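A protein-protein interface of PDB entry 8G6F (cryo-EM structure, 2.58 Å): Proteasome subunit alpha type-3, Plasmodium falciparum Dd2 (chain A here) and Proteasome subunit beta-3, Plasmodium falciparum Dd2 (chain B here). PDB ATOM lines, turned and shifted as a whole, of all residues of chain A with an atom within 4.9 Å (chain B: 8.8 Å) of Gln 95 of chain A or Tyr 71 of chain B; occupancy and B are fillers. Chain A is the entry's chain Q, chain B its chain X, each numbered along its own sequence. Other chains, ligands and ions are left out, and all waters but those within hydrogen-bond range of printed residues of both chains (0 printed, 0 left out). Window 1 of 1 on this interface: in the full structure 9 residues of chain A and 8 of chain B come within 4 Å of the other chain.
The side-chain amide nitrogen (ND2) of Asn 74 of chain B is in hydrogen-bond range of the side-chain amide oxygen (OE1) of Gln 95 of chain A.
The side-chain carboxylate (OD2) of Asp 69 of chain A sits at hydrogen-bond distance from the side-chain amide nitrogen (NE2) of Gln 95 of chain A.
Among the printed residues, pairs that only touch across the chains: Arg 91 of chain A with Val 78 of chain B, Leu 92 of chain A with Tyr 71 of chain B, Leu 92 of chain A with Leu 75 of chain B, Gln 95 of chain A with Tyr 71 of chain B, Gln 95 of chain A with Leu 75 of chain B, Arg 96 of chain A with Tyr 71 of chain B, Leu 98 of chain A with Arg 70 of chain B, Leu 98 of chain A with Asn 74 of chain B, Tyr 99 of chain A with Glu 67 of chain B and Tyr 99 of chain A with Ile 68 of chain B.
Asp 69 of chain A touches none of the printed residues of chain B. Printed residues of chain B within 4 Å of Arg 91 of chain A: Val 78. Of the printed residues of chain B, Gln 95 of chain A touches Tyr 71 (3.5 Å), Asn 74 (2.9 Å) and Leu 75 (3.8 Å). Printed residues of chain B within 4 Å of Arg 96 of chain A: Tyr 71. Tyr 71 of chain B touches three residues of chain A. The nearest printed residue of chain A that does not touch Arg 70 of chain B is Gln 95 of chain A (4.2 Å).
Of the 21 printed residues of chain B, 7 touch a printed residue of chain A. Hydrophobic or aromatic side chains of chain A within 4 Å of the printed part of chain B: Leu 92, Leu 98 and Tyr 99. Among the printed residues, no Asp or Glu carboxylate lies within 4 Å of a Lys or Arg side-chain nitrogen of the other chain.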
ATOM      1  N   ASP A  69      29.657  24.849   0.271  1.00  0.00           N
ATOM      2  CA  ASP A  69      29.145  23.490   0.221  1.00  0.00           C
ATOM      3  C   ASP A  69      30.332  22.554   0.367  1.00  0.00           C
ATOM      4  O   ASP A  69      31.476  22.992   0.507  1.00  0.00           O
ATOM      5  CB  ASP A  69      28.386  23.233  -1.079  1.00  0.00           C
ATOM      6  CG  ASP A  69      27.193  22.331  -0.882  1.00  0.00           C
ATOM      7  OD1 ASP A  69      27.379  21.102  -0.784  1.00  0.00           O
ATOM      8  OD2 ASP A  69      26.064  22.853  -0.818  1.00  0.00           O
ATOM      9  N   ARG A  91      24.880  29.573   0.132  1.00  0.00           N
ATOM     10  CA  ARG A  91      24.636  28.301   0.801  1.00  0.00           C
ATOM     11  C   ARG A  91      23.192  27.861   0.615  1.00  0.00           C
ATOM     12  O   ARG A  91      22.918  26.684   0.332  1.00  0.00           O
ATOM     13  CB  ARG A  91      24.991  28.426   2.279  1.00  0.00           C
ATOM     14  CG  ARG A  91      26.471  28.624   2.517  1.00  0.00           C
ATOM     15  CD  ARG A  91      26.766  29.020   3.939  1.00  0.00           C
ATOM     16  NE  ARG A  91      28.180  28.879   4.245  1.00  0.00           N
ATOM     17  CZ  ARG A  91      28.770  29.375   5.322  1.00  0.00           C
ATOM     18  NH1 ARG A  91      28.092  30.048   6.233  1.00  0.00           N
ATOM     19  NH2 ARG A  91      30.075  29.189   5.489  1.00  0.00           N
ATOM     20  N   LEU A  92      22.254  28.800   0.746  1.00  0.00           N
ATOM     21  CA  LEU A  92      20.856  28.483   0.482  1.00  0.00           C
ATOM     22  C   LEU A  92      20.662  28.009  -0.950  1.00  0.00           C
ATOM     23  O   LEU A  92      19.902  27.073  -1.200  1.00  0.00           O
ATOM     24  CB  LEU A  92      19.979  29.703   0.753  1.00  0.00           C
ATOM     25  CG  LEU A  92      19.592  29.953   2.207  1.00  0.00           C
ATOM     26  CD1 LEU A  92      19.007  31.342   2.352  1.00  0.00           C
ATOM     27  CD2 LEU A  92      18.611  28.910   2.686  1.00  0.00           C
ATOM     28  N   TYR A  93      21.325  28.655  -1.907  1.00  0.00           N
ATOM     29  CA  TYR A  93      21.158  28.284  -3.309  1.00  0.00           C
ATOM     30  C   TYR A  93      21.677  26.881  -3.577  1.00  0.00           C
ATOM     31  O   TYR A  93      21.033  26.098  -4.288  1.00  0.00           O
ATOM     32  CB  TYR A  93      21.881  29.282  -4.209  1.00  0.00           C
ATOM     33  CG  TYR A  93      21.136  30.567  -4.476  1.00  0.00           C
ATOM     34  CD1 TYR A  93      19.762  30.579  -4.648  1.00  0.00           C
ATOM     35  CD2 TYR A  93      21.813  31.770  -4.570  1.00  0.00           C
ATOM     36  CE1 TYR A  93      19.087  31.746  -4.894  1.00  0.00           C
ATOM     37  CE2 TYR A  93      21.145  32.943  -4.817  1.00  0.00           C
ATOM     38  CZ  TYR A  93      19.780  32.926  -4.976  1.00  0.00           C
ATOM     39  OH  TYR A  93      19.104  34.095  -5.225  1.00  0.00           O
ATOM     40  N   ALA A  94      22.851  26.550  -3.043  1.00  0.00           N
ATOM     41  CA  ALA A  94      23.398  25.214  -3.251  1.00  0.00           C
ATOM     42  C   ALA A  94      22.494  24.155  -2.638  1.00  0.00           C
ATOM     43  O   ALA A  94      22.218  23.119  -3.261  1.00  0.00           O
ATOM     44  CB  ALA A  94      24.807  25.128  -2.669  1.00  0.00           C
ATOM     45  N   GLN A  95      21.998  24.404  -1.425  1.00  0.00           N
ATOM     46  CA  GLN A  95      21.110  23.428  -0.812  1.00  0.00           C
ATOM     47  C   GLN A  95      19.787  23.329  -1.558  1.00  0.00           C
ATOM     48  O   GLN A  95      19.210  22.243  -1.646  1.00  0.00           O
ATOM     49  CB  GLN A  95      20.881  23.775   0.658  1.00  0.00           C
ATOM     50  CG  GLN A  95      22.023  23.394   1.587  1.00  0.00           C
ATOM     51  CD  GLN A  95      22.688  22.091   1.213  1.00  0.00           C
ATOM     52  OE1 GLN A  95      22.086  21.026   1.311  1.00  0.00           O
ATOM     53  NE2 GLN A  95      23.932  22.167   0.772  1.00  0.00           N
ATOM     54  N   ARG A  96      19.295  24.440  -2.105  1.00  0.00           N
ATOM     55  CA  ARG A  96      18.071  24.405  -2.895  1.00  0.00           C
ATOM     56  C   ARG A  96      18.259  23.583  -4.161  1.00  0.00           C
ATOM     57  O   ARG A  96      17.367  22.827  -4.554  1.00  0.00           O
ATOM     58  CB  ARG A  96      17.636  25.828  -3.233  1.00  0.00           C
ATOM     59  CG  ARG A  96      16.294  25.930  -3.927  1.00  0.00           C
ATOM     60  CD  ARG A  96      15.168  26.052  -2.926  1.00  0.00           C
ATOM     61  NE  ARG A  96      13.888  25.649  -3.496  1.00  0.00           N
ATOM     62  CZ  ARG A  96      12.841  25.252  -2.786  1.00  0.00           C
ATOM     63  NH1 ARG A  96      12.882  25.195  -1.465  1.00  0.00           N
ATOM     64  NH2 ARG A  96      11.723  24.907  -3.417  1.00  0.00           N
ATOM     65  N   TYR A  97      19.407  23.724  -4.825  1.00  0.00           N
ATOM     66  CA  TYR A  97      19.665  22.899  -5.999  1.00  0.00           C
ATOM     67  C   TYR A  97      19.716  21.425  -5.633  1.00  0.00           C
ATOM     68  O   TYR A  97      19.178  20.580  -6.357  1.00  0.00           O
ATOM     69  CB  TYR A  97      20.969  23.314  -6.673  1.00  0.00           C
ATOM     70  CG  TYR A  97      21.251  22.569  -7.957  1.00  0.00           C
ATOM     71  CD1 TYR A  97      21.728  21.267  -7.940  1.00  0.00           C
ATOM     72  CD2 TYR A  97      21.042  23.166  -9.188  1.00  0.00           C
ATOM     73  CE1 TYR A  97      21.980  20.583  -9.108  1.00  0.00           C
ATOM     74  CE2 TYR A  97      21.297  22.490 -10.363  1.00  0.00           C
ATOM     75  CZ  TYR A  97      21.765  21.201 -10.314  1.00  0.00           C
ATOM     76  OH  TYR A  97      22.022  20.523 -11.478  1.00  0.00           O
ATOM     77  N   LEU A  98      20.387  21.088  -4.531  1.00  0.00           N
ATOM     78  CA  LEU A  98      20.425  19.689  -4.119  1.00  0.00           C
ATOM     79  C   LEU A  98      19.023  19.180  -3.815  1.00  0.00           C
ATOM     80  O   LEU A  98      18.669  18.055  -4.176  1.00  0.00           O
ATOM     81  CB  LEU A  98      21.343  19.519  -2.910  1.00  0.00           C
ATOM     82  CG  LEU A  98      21.404  18.127  -2.278  1.00  0.00           C
ATOM     83  CD1 LEU A  98      21.719  17.061  -3.302  1.00  0.00           C
ATOM     84  CD2 LEU A  98      22.425  18.101  -1.168  1.00  0.00           C
ATOM     85  N   TYR A  99      18.203  20.009  -3.176  1.00  0.00           N
ATOM     86  CA  TYR A  99      16.823  19.637  -2.888  1.00  0.00           C
ATOM     87  C   TYR A  99      16.032  19.401  -4.169  1.00  0.00           C
ATOM     88  O   TYR A  99      15.223  18.471  -4.246  1.00  0.00           O
ATOM     89  CB  TYR A  99      16.188  20.738  -2.040  1.00  0.00           C
ATOM     90  CG  TYR A  99      14.707  20.614  -1.808  1.00  0.00           C
ATOM     91  CD1 TYR A  99      14.212  19.859  -0.760  1.00  0.00           C
ATOM     92  CD2 TYR A  99      13.802  21.280  -2.618  1.00  0.00           C
ATOM     93  CE1 TYR A  99      12.859  19.752  -0.537  1.00  0.00           C
ATOM     94  CE2 TYR A  99      12.447  21.179  -2.404  1.00  0.00           C
ATOM     95  CZ  TYR A  99      11.981  20.415  -1.360  1.00  0.00           C
ATOM     96  OH  TYR A  99      10.629  20.311  -1.139  1.00  0.00           O
ATOM     97  N   MET B  47      22.252  11.008   7.914  1.00  0.00           N
ATOM     98  CA  MET B  47      22.277  12.460   8.002  1.00  0.00           C
ATOM     99  C   MET B  47      23.691  12.970   8.244  1.00  0.00           C
ATOM    100  O   MET B  47      24.132  13.924   7.599  1.00  0.00           O
ATOM    101  CB  MET B  47      21.338  12.925   9.113  1.00  0.00           C
ATOM    102  CG  MET B  47      19.872  12.802   8.749  1.00  0.00           C
ATOM    103  SD  MET B  47      19.422  13.805   7.323  1.00  0.00           S
ATOM    104  CE  MET B  47      18.562  12.606   6.323  1.00  0.00           C
ATOM    105  N   THR B  64      10.306  12.898  -0.013  1.00  0.00           N
ATOM    106  CA  THR B  64      10.158  14.323   0.260  1.00  0.00           C
ATOM    107  C   THR B  64      10.733  14.686   1.623  1.00  0.00           C
ATOM    108  O   THR B  64      11.479  15.665   1.757  1.00  0.00           O
ATOM    109  CB  THR B  64       8.683  14.709   0.187  1.00  0.00           C
ATOM    110  OG1 THR B  64       8.201  14.512  -1.143  1.00  0.00           O
ATOM    111  CG2 THR B  64       8.488  16.157   0.583  1.00  0.00           C
ATOM    112  N   LEU B  65      10.388  13.913   2.654  1.00  0.00           N
ATOM    113  CA  LEU B  65      10.892  14.195   3.989  1.00  0.00           C
ATOM    114  C   LEU B  65      12.402  14.051   4.044  1.00  0.00           C
ATOM    115  O   LEU B  65      13.078  14.830   4.718  1.00  0.00           O
ATOM    116  CB  LEU B  65      10.226  13.271   5.008  1.00  0.00           C
ATOM    117  CG  LEU B  65      10.491  13.609   6.474  1.00  0.00           C
ATOM    118  CD1 LEU B  65       9.890  14.950   6.830  1.00  0.00           C
ATOM    119  CD2 LEU B  65       9.951  12.533   7.386  1.00  0.00           C
ATOM    120  N   TYR B  66      12.954  13.057   3.349  1.00  0.00           N
ATOM    121  CA  TYR B  66      14.403  12.913   3.328  1.00  0.00           C
ATOM    122  C   TYR B  66      15.064  14.116   2.679  1.00  0.00           C
ATOM    123  O   TYR B  66      16.097  14.593   3.153  1.00  0.00           O
ATOM    124  CB  TYR B  66      14.809  11.642   2.593  1.00  0.00           C
ATOM    125  CG  TYR B  66      16.282  11.619   2.269  1.00  0.00           C
ATOM    126  CD1 TYR B  66      17.228  11.708   3.275  1.00  0.00           C
ATOM    127  CD2 TYR B  66      16.725  11.531   0.962  1.00  0.00           C
ATOM    128  CE1 TYR B  66      18.571  11.700   2.990  1.00  0.00           C
ATOM    129  CE2 TYR B  66      18.067  11.520   0.668  1.00  0.00           C
ATOM    130  CZ  TYR B  66      18.985  11.605   1.687  1.00  0.00           C
ATOM    131  OH  TYR B  66      20.328  11.593   1.404  1.00  0.00           O
ATOM    132  N   GLU B  67      14.500  14.608   1.576  1.00  0.00           N
ATOM    133  CA  GLU B  67      15.082  15.774   0.924  1.00  0.00           C
ATOM    134  C   GLU B  67      15.028  16.993   1.835  1.00  0.00           C
ATOM    135  O   GLU B  67      16.001  17.750   1.935  1.00  0.00           O
ATOM    136  CB  GLU B  67      14.365  16.044  -0.397  1.00  0.00           C
ATOM    137  CG  GLU B  67      14.740  15.064  -1.493  1.00  0.00           C
ATOM    138  CD  GLU B  67      13.672  14.927  -2.569  1.00  0.00           C
ATOM    139  OE1 GLU B  67      12.585  15.524  -2.424  1.00  0.00           O
ATOM    140  OE2 GLU B  67      13.926  14.223  -3.566  1.00  0.00           O
ATOM    141  N   ILE B  68      13.906  17.187   2.528  1.00  0.00           N
ATOM    142  CA  ILE B  68      13.790  18.314   3.452  1.00  0.00           C
ATOM    143  C   ILE B  68      14.807  18.186   4.578  1.00  0.00           C
ATOM    144  O   ILE B  68      15.468  19.158   4.960  1.00  0.00           O
ATOM    145  CB  ILE B  68      12.357  18.409   4.005  1.00  0.00           C
ATOM    146  CG1 ILE B  68      11.378  18.784   2.896  1.00  0.00           C
ATOM    147  CG2 ILE B  68      12.290  19.424   5.134  1.00  0.00           C
ATOM    148  CD1 ILE B  68       9.945  18.493   3.238  1.00  0.00           C
ATOM    149  N   LEU B  69      14.929  16.986   5.145  1.00  0.00           N
ATOM    150  CA  LEU B  69      15.839  16.781   6.264  1.00  0.00           C
ATOM    151  C   LEU B  69      17.285  16.972   5.839  1.00  0.00           C
ATOM    152  O   LEU B  69      18.079  17.553   6.580  1.00  0.00           O
ATOM    153  CB  LEU B  69      15.638  15.387   6.855  1.00  0.00           C
ATOM    154  CG  LEU B  69      14.311  15.141   7.572  1.00  0.00           C
ATOM    155  CD1 LEU B  69      14.143  13.668   7.876  1.00  0.00           C
ATOM    156  CD2 LEU B  69      14.232  15.960   8.841  1.00  0.00           C
ATOM    157  N   ARG B  70      17.650  16.475   4.659  1.00  0.00           N
ATOM    158  CA  ARG B  70      19.000  16.686   4.157  1.00  0.00           C
ATOM    159  C   ARG B  70      19.274  18.167   3.945  1.00  0.00           C
ATOM    160  O   ARG B  70      20.346  18.663   4.299  1.00  0.00           O
ATOM    161  CB  ARG B  70      19.197  15.906   2.860  1.00  0.00           C
ATOM    162  CG  ARG B  70      20.590  16.004   2.282  1.00  0.00           C
ATOM    163  CD  ARG B  70      20.709  15.217   1.000  1.00  0.00           C
ATOM    164  NE  ARG B  70      19.670  15.580   0.047  1.00  0.00           N
ATOM    165  CZ  ARG B  70      19.422  14.924  -1.077  1.00  0.00           C
ATOM    166  NH1 ARG B  70      20.127  13.864  -1.426  1.00  0.00           N
ATOM    167  NH2 ARG B  70      18.444  15.345  -1.871  1.00  0.00           N
ATOM    168  N   TYR B  71      18.309  18.890   3.381  1.00  0.00           N
ATOM    169  CA  TYR B  71      18.459  20.330   3.209  1.00  0.00           C
ATOM    170  C   TYR B  71      18.724  21.015   4.543  1.00  0.00           C
ATOM    171  O   TYR B  71      19.692  21.773   4.694  1.00  0.00           O
ATOM    172  CB  TYR B  71      17.195  20.874   2.544  1.00  0.00           C
ATOM    173  CG  TYR B  71      17.092  22.371   2.425  1.00  0.00           C
ATOM    174  CD1 TYR B  71      16.602  23.138   3.467  1.00  0.00           C
ATOM    175  CD2 TYR B  71      17.442  23.011   1.254  1.00  0.00           C
ATOM    176  CE1 TYR B  71      16.495  24.501   3.352  1.00  0.00           C
ATOM    177  CE2 TYR B  71      17.338  24.370   1.130  1.00  0.00           C
ATOM    178  CZ  TYR B  71      16.863  25.111   2.178  1.00  0.00           C
ATOM    179  OH  TYR B  71      16.758  26.473   2.050  1.00  0.00           O
ATOM    180  N   ARG B  72      17.876  20.739   5.534  1.00  0.00           N
ATOM    181  CA  ARG B  72      17.999  21.393   6.831  1.00  0.00           C
ATOM    182  C   ARG B  72      19.315  21.041   7.508  1.00  0.00           C
ATOM    183  O   ARG B  72      20.002  21.915   8.049  1.00  0.00           O
ATOM    184  CB  ARG B  72      16.821  21.001   7.718  1.00  0.00           C
ATOM    185  CG  ARG B  72      15.479  21.495   7.220  1.00  0.00           C
ATOM    186  CD  ARG B  72      15.310  22.980   7.452  1.00  0.00           C
ATOM    187  NE  ARG B  72      15.470  23.336   8.856  1.00  0.00           N
ATOM    188  CZ  ARG B  72      14.475  23.451   9.725  1.00  0.00           C
ATOM    189  NH1 ARG B  72      13.218  23.245   9.372  1.00  0.00           N
ATOM    190  NH2 ARG B  72      14.751  23.778  10.983  1.00  0.00           N
ATOM    191  N   VAL B  73      19.681  19.760   7.499  1.00  0.00           N
ATOM    192  CA  VAL B  73      20.900  19.331   8.174  1.00  0.00           C
ATOM    193  C   VAL B  73      22.121  19.938   7.501  1.00  0.00           C
ATOM    194  O   VAL B  73      23.054  20.388   8.172  1.00  0.00           O
ATOM    195  CB  VAL B  73      20.978  17.793   8.210  1.00  0.00           C
ATOM    196  CG1 VAL B  73      22.372  17.334   8.575  1.00  0.00           C
ATOM    197  CG2 VAL B  73      19.975  17.241   9.193  1.00  0.00           C
ATOM    198  N   ASN B  74      22.145  19.949   6.167  1.00  0.00           N
ATOM    199  CA  ASN B  74      23.286  20.514   5.462  1.00  0.00           C
ATOM    200  C   ASN B  74      23.429  21.998   5.750  1.00  0.00           C
ATOM    201  O   ASN B  74      24.542  22.486   5.974  1.00  0.00           O
ATOM    202  CB  ASN B  74      23.141  20.272   3.962  1.00  0.00           C
ATOM    203  CG  ASN B  74      23.520  18.868   3.562  1.00  0.00           C
ATOM    204  OD1 ASN B  74      23.936  18.066   4.392  1.00  0.00           O
ATOM    205  ND2 ASN B  74      23.378  18.562   2.284  1.00  0.00           N
ATOM    206  N   LEU B  75      22.320  22.737   5.750  1.00  0.00           N
ATOM    207  CA  LEU B  75      22.401  24.161   6.054  1.00  0.00           C
ATOM    208  C   LEU B  75      22.889  24.390   7.476  1.00  0.00           C
ATOM    209  O   LEU B  75      23.775  25.219   7.720  1.00  0.00           O
ATOM    210  CB  LEU B  75      21.043  24.819   5.842  1.00  0.00           C
ATOM    211  CG  LEU B  75      20.922  25.556   4.513  1.00  0.00           C
ATOM    212  CD1 LEU B  75      19.470  25.693   4.133  1.00  0.00           C
ATOM    213  CD2 LEU B  75      21.593  26.916   4.595  1.00  0.00           C
ATOM    214  N   TYR B  76      22.327  23.655   8.434  1.00  0.00           N
ATOM    215  CA  TYR B  76      22.746  23.803   9.821  1.00  0.00           C
ATOM    216  C   TYR B  76      24.235  23.526   9.966  1.00  0.00           C
ATOM    217  O   TYR B  76      24.959  24.279  10.624  1.00  0.00           O
ATOM    218  CB  TYR B  76      21.922  22.858  10.697  1.00  0.00           C
ATOM    219  CG  TYR B  76      22.217  22.916  12.176  1.00  0.00           C
ATOM    220  CD1 TYR B  76      23.368  22.347  12.698  1.00  0.00           C
ATOM    221  CD2 TYR B  76      21.330  23.516  13.053  1.00  0.00           C
ATOM    222  CE1 TYR B  76      23.635  22.392  14.043  1.00  0.00           C
ATOM    223  CE2 TYR B  76      21.587  23.563  14.401  1.00  0.00           C
ATOM    224  CZ  TYR B  76      22.738  22.998  14.893  1.00  0.00           C
ATOM    225  OH  TYR B  76      22.998  23.044  16.239  1.00  0.00           O
ATOM    226  N   GLU B  77      24.712  22.450   9.341  1.00  0.00           N
ATOM    227  CA  GLU B  77      26.096  22.039   9.529  1.00  0.00           C
ATOM    228  C   GLU B  77      27.060  22.990   8.835  1.00  0.00           C
ATOM    229  O   GLU B  77      28.135  23.278   9.369  1.00  0.00           O
ATOM    230  CB  GLU B  77      26.283  20.610   9.028  1.00  0.00           C
ATOM    231  CG  GLU B  77      25.565  19.586   9.882  1.00  0.00           C
ATOM    232  CD  GLU B  77      25.793  18.161   9.427  1.00  0.00           C
ATOM    233  OE1 GLU B  77      25.893  17.927   8.207  1.00  0.00           O
ATOM    234  OE2 GLU B  77      25.860  17.267  10.291  1.00  0.00           O
ATOM    235  N   VAL B  78      26.705  23.496   7.654  1.00  0.00           N
ATOM    236  CA  VAL B  78      27.587  24.446   6.987  1.00  0.00           C
ATOM    237  C   VAL B  78      27.636  25.757   7.761  1.00  0.00           C
ATOM    238  O   VAL B  78      28.688  26.397   7.850  1.00  0.00           O
ATOM    239  CB  VAL B  78      27.158  24.658   5.523  1.00  0.00           C
ATOM    240  CG1 VAL B  78      25.989  25.617   5.423  1.00  0.00           C
ATOM    241  CG2 VAL B  78      28.331  25.163   4.698  1.00  0.00           C
ATOM    242  N   ARG B  79      26.507  26.176   8.337  1.00  0.00           N
ATOM    243  CA  ARG B  79      26.496  27.419   9.101  1.00  0.00           C
ATOM    244  C   ARG B  79      27.306  27.288  10.384  1.00  0.00           C
ATOM    245  O   ARG B  79      28.099  28.173  10.720  1.00  0.00           O
ATOM    246  CB  ARG B  79      25.057  27.823   9.413  1.00  0.00           C
ATOM    247  CG  ARG B  79      24.367  28.557   8.282  1.00  0.00           C
ATOM    248  CD  ARG B  79      22.966  28.987   8.663  1.00  0.00           C
ATOM    249  NE  ARG B  79      22.962  29.910   9.792  1.00  0.00           N
ATOM    250  CZ  ARG B  79      22.935  31.233   9.693  1.00  0.00           C
ATOM    251  NH1 ARG B  79      22.910  31.842   8.520  1.00  0.00           N
ATOM    252  NH2 ARG B  79      22.935  31.966  10.802  1.00  0.00           N
ATOM    253  N   MET B  84      25.692  18.041  13.259  1.00  0.00           N
ATOM    254  CA  MET B  84      24.470  18.260  14.017  1.00  0.00           C
ATOM    255  C   MET B  84      24.319  17.208  15.106  1.00  0.00           C
ATOM    256  O   MET B  84      24.565  16.020  14.885  1.00  0.00           O
ATOM    257  CB  MET B  84      23.260  18.230  13.090  1.00  0.00           C
ATOM    258  CG  MET B  84      21.968  18.655  13.749  1.00  0.00           C
ATOM    259  SD  MET B  84      20.635  18.862  12.566  1.00  0.00           S
ATOM    260  CE  MET B  84      19.645  20.079  13.406  1.00  0.00           C
ATOM    261  N   PHE B  89      18.727  17.079  15.986  1.00  0.00           N
ATOM    262  CA  PHE B  89      18.065  16.564  14.796  1.00  0.00           C
ATOM    263  C   PHE B  89      16.712  15.958  15.137  1.00  0.00           C
ATOM    264  O   PHE B  89      15.751  16.108  14.377  1.00  0.00           O
ATOM    265  CB  PHE B  89      18.938  15.526  14.098  1.00  0.00           C
ATOM    266  CG  PHE B  89      18.273  14.901  12.914  1.00  0.00           C
ATOM    267  CD1 PHE B  89      18.294  15.529  11.687  1.00  0.00           C
ATOM    268  CD2 PHE B  89      17.593  13.706  13.035  1.00  0.00           C
ATOM    269  CE1 PHE B  89      17.669  14.972  10.604  1.00  0.00           C
ATOM    270  CE2 PHE B  89      16.966  13.148  11.952  1.00  0.00           C
ATOM    271  CZ  PHE B  89      17.004  13.783  10.735  1.00  0.00           C
ATOM    272  N   MET B  92      14.293  18.792  15.670  1.00  0.00           N
ATOM    273  CA  MET B  92      13.989  19.426  14.394  1.00  0.00           C
ATOM    274  C   MET B  92      13.040  18.568  13.572  1.00  0.00           C
ATOM    275  O   MET B  92      12.136  19.088  12.914  1.00  0.00           O
ATOM    276  CB  MET B  92      15.281  19.693  13.625  1.00  0.00           C
ATOM    277  CG  MET B  92      15.079  20.199  12.209  1.00  0.00           C
ATOM    278  SD  MET B  92      16.621  20.342  11.308  1.00  0.00           S
ATOM    279  CE  MET B  92      16.703  18.728  10.552  1.00  0.00           C
ATOM    280  N   ILE B  96       9.414  19.720  12.238  1.00  0.00           N
ATOM    281  CA  ILE B  96       9.088  19.658  10.817  1.00  0.00           C
ATOM    282  C   ILE B  96       7.829  18.833  10.598  1.00  0.00           C
ATOM    283  O   ILE B  96       6.949  19.212   9.818  1.00  0.00           O
ATOM    284  CB  ILE B  96      10.275  19.091  10.018  1.00  0.00           C
ATOM    285  CG1 ILE B  96      11.375  20.138   9.873  1.00  0.00           C
ATOM    286  CG2 ILE B  96       9.824  18.623   8.646  1.00  0.00           C
ATOM    287  CD1 ILE B  96      12.716  19.556   9.521  1.00  0.00           C
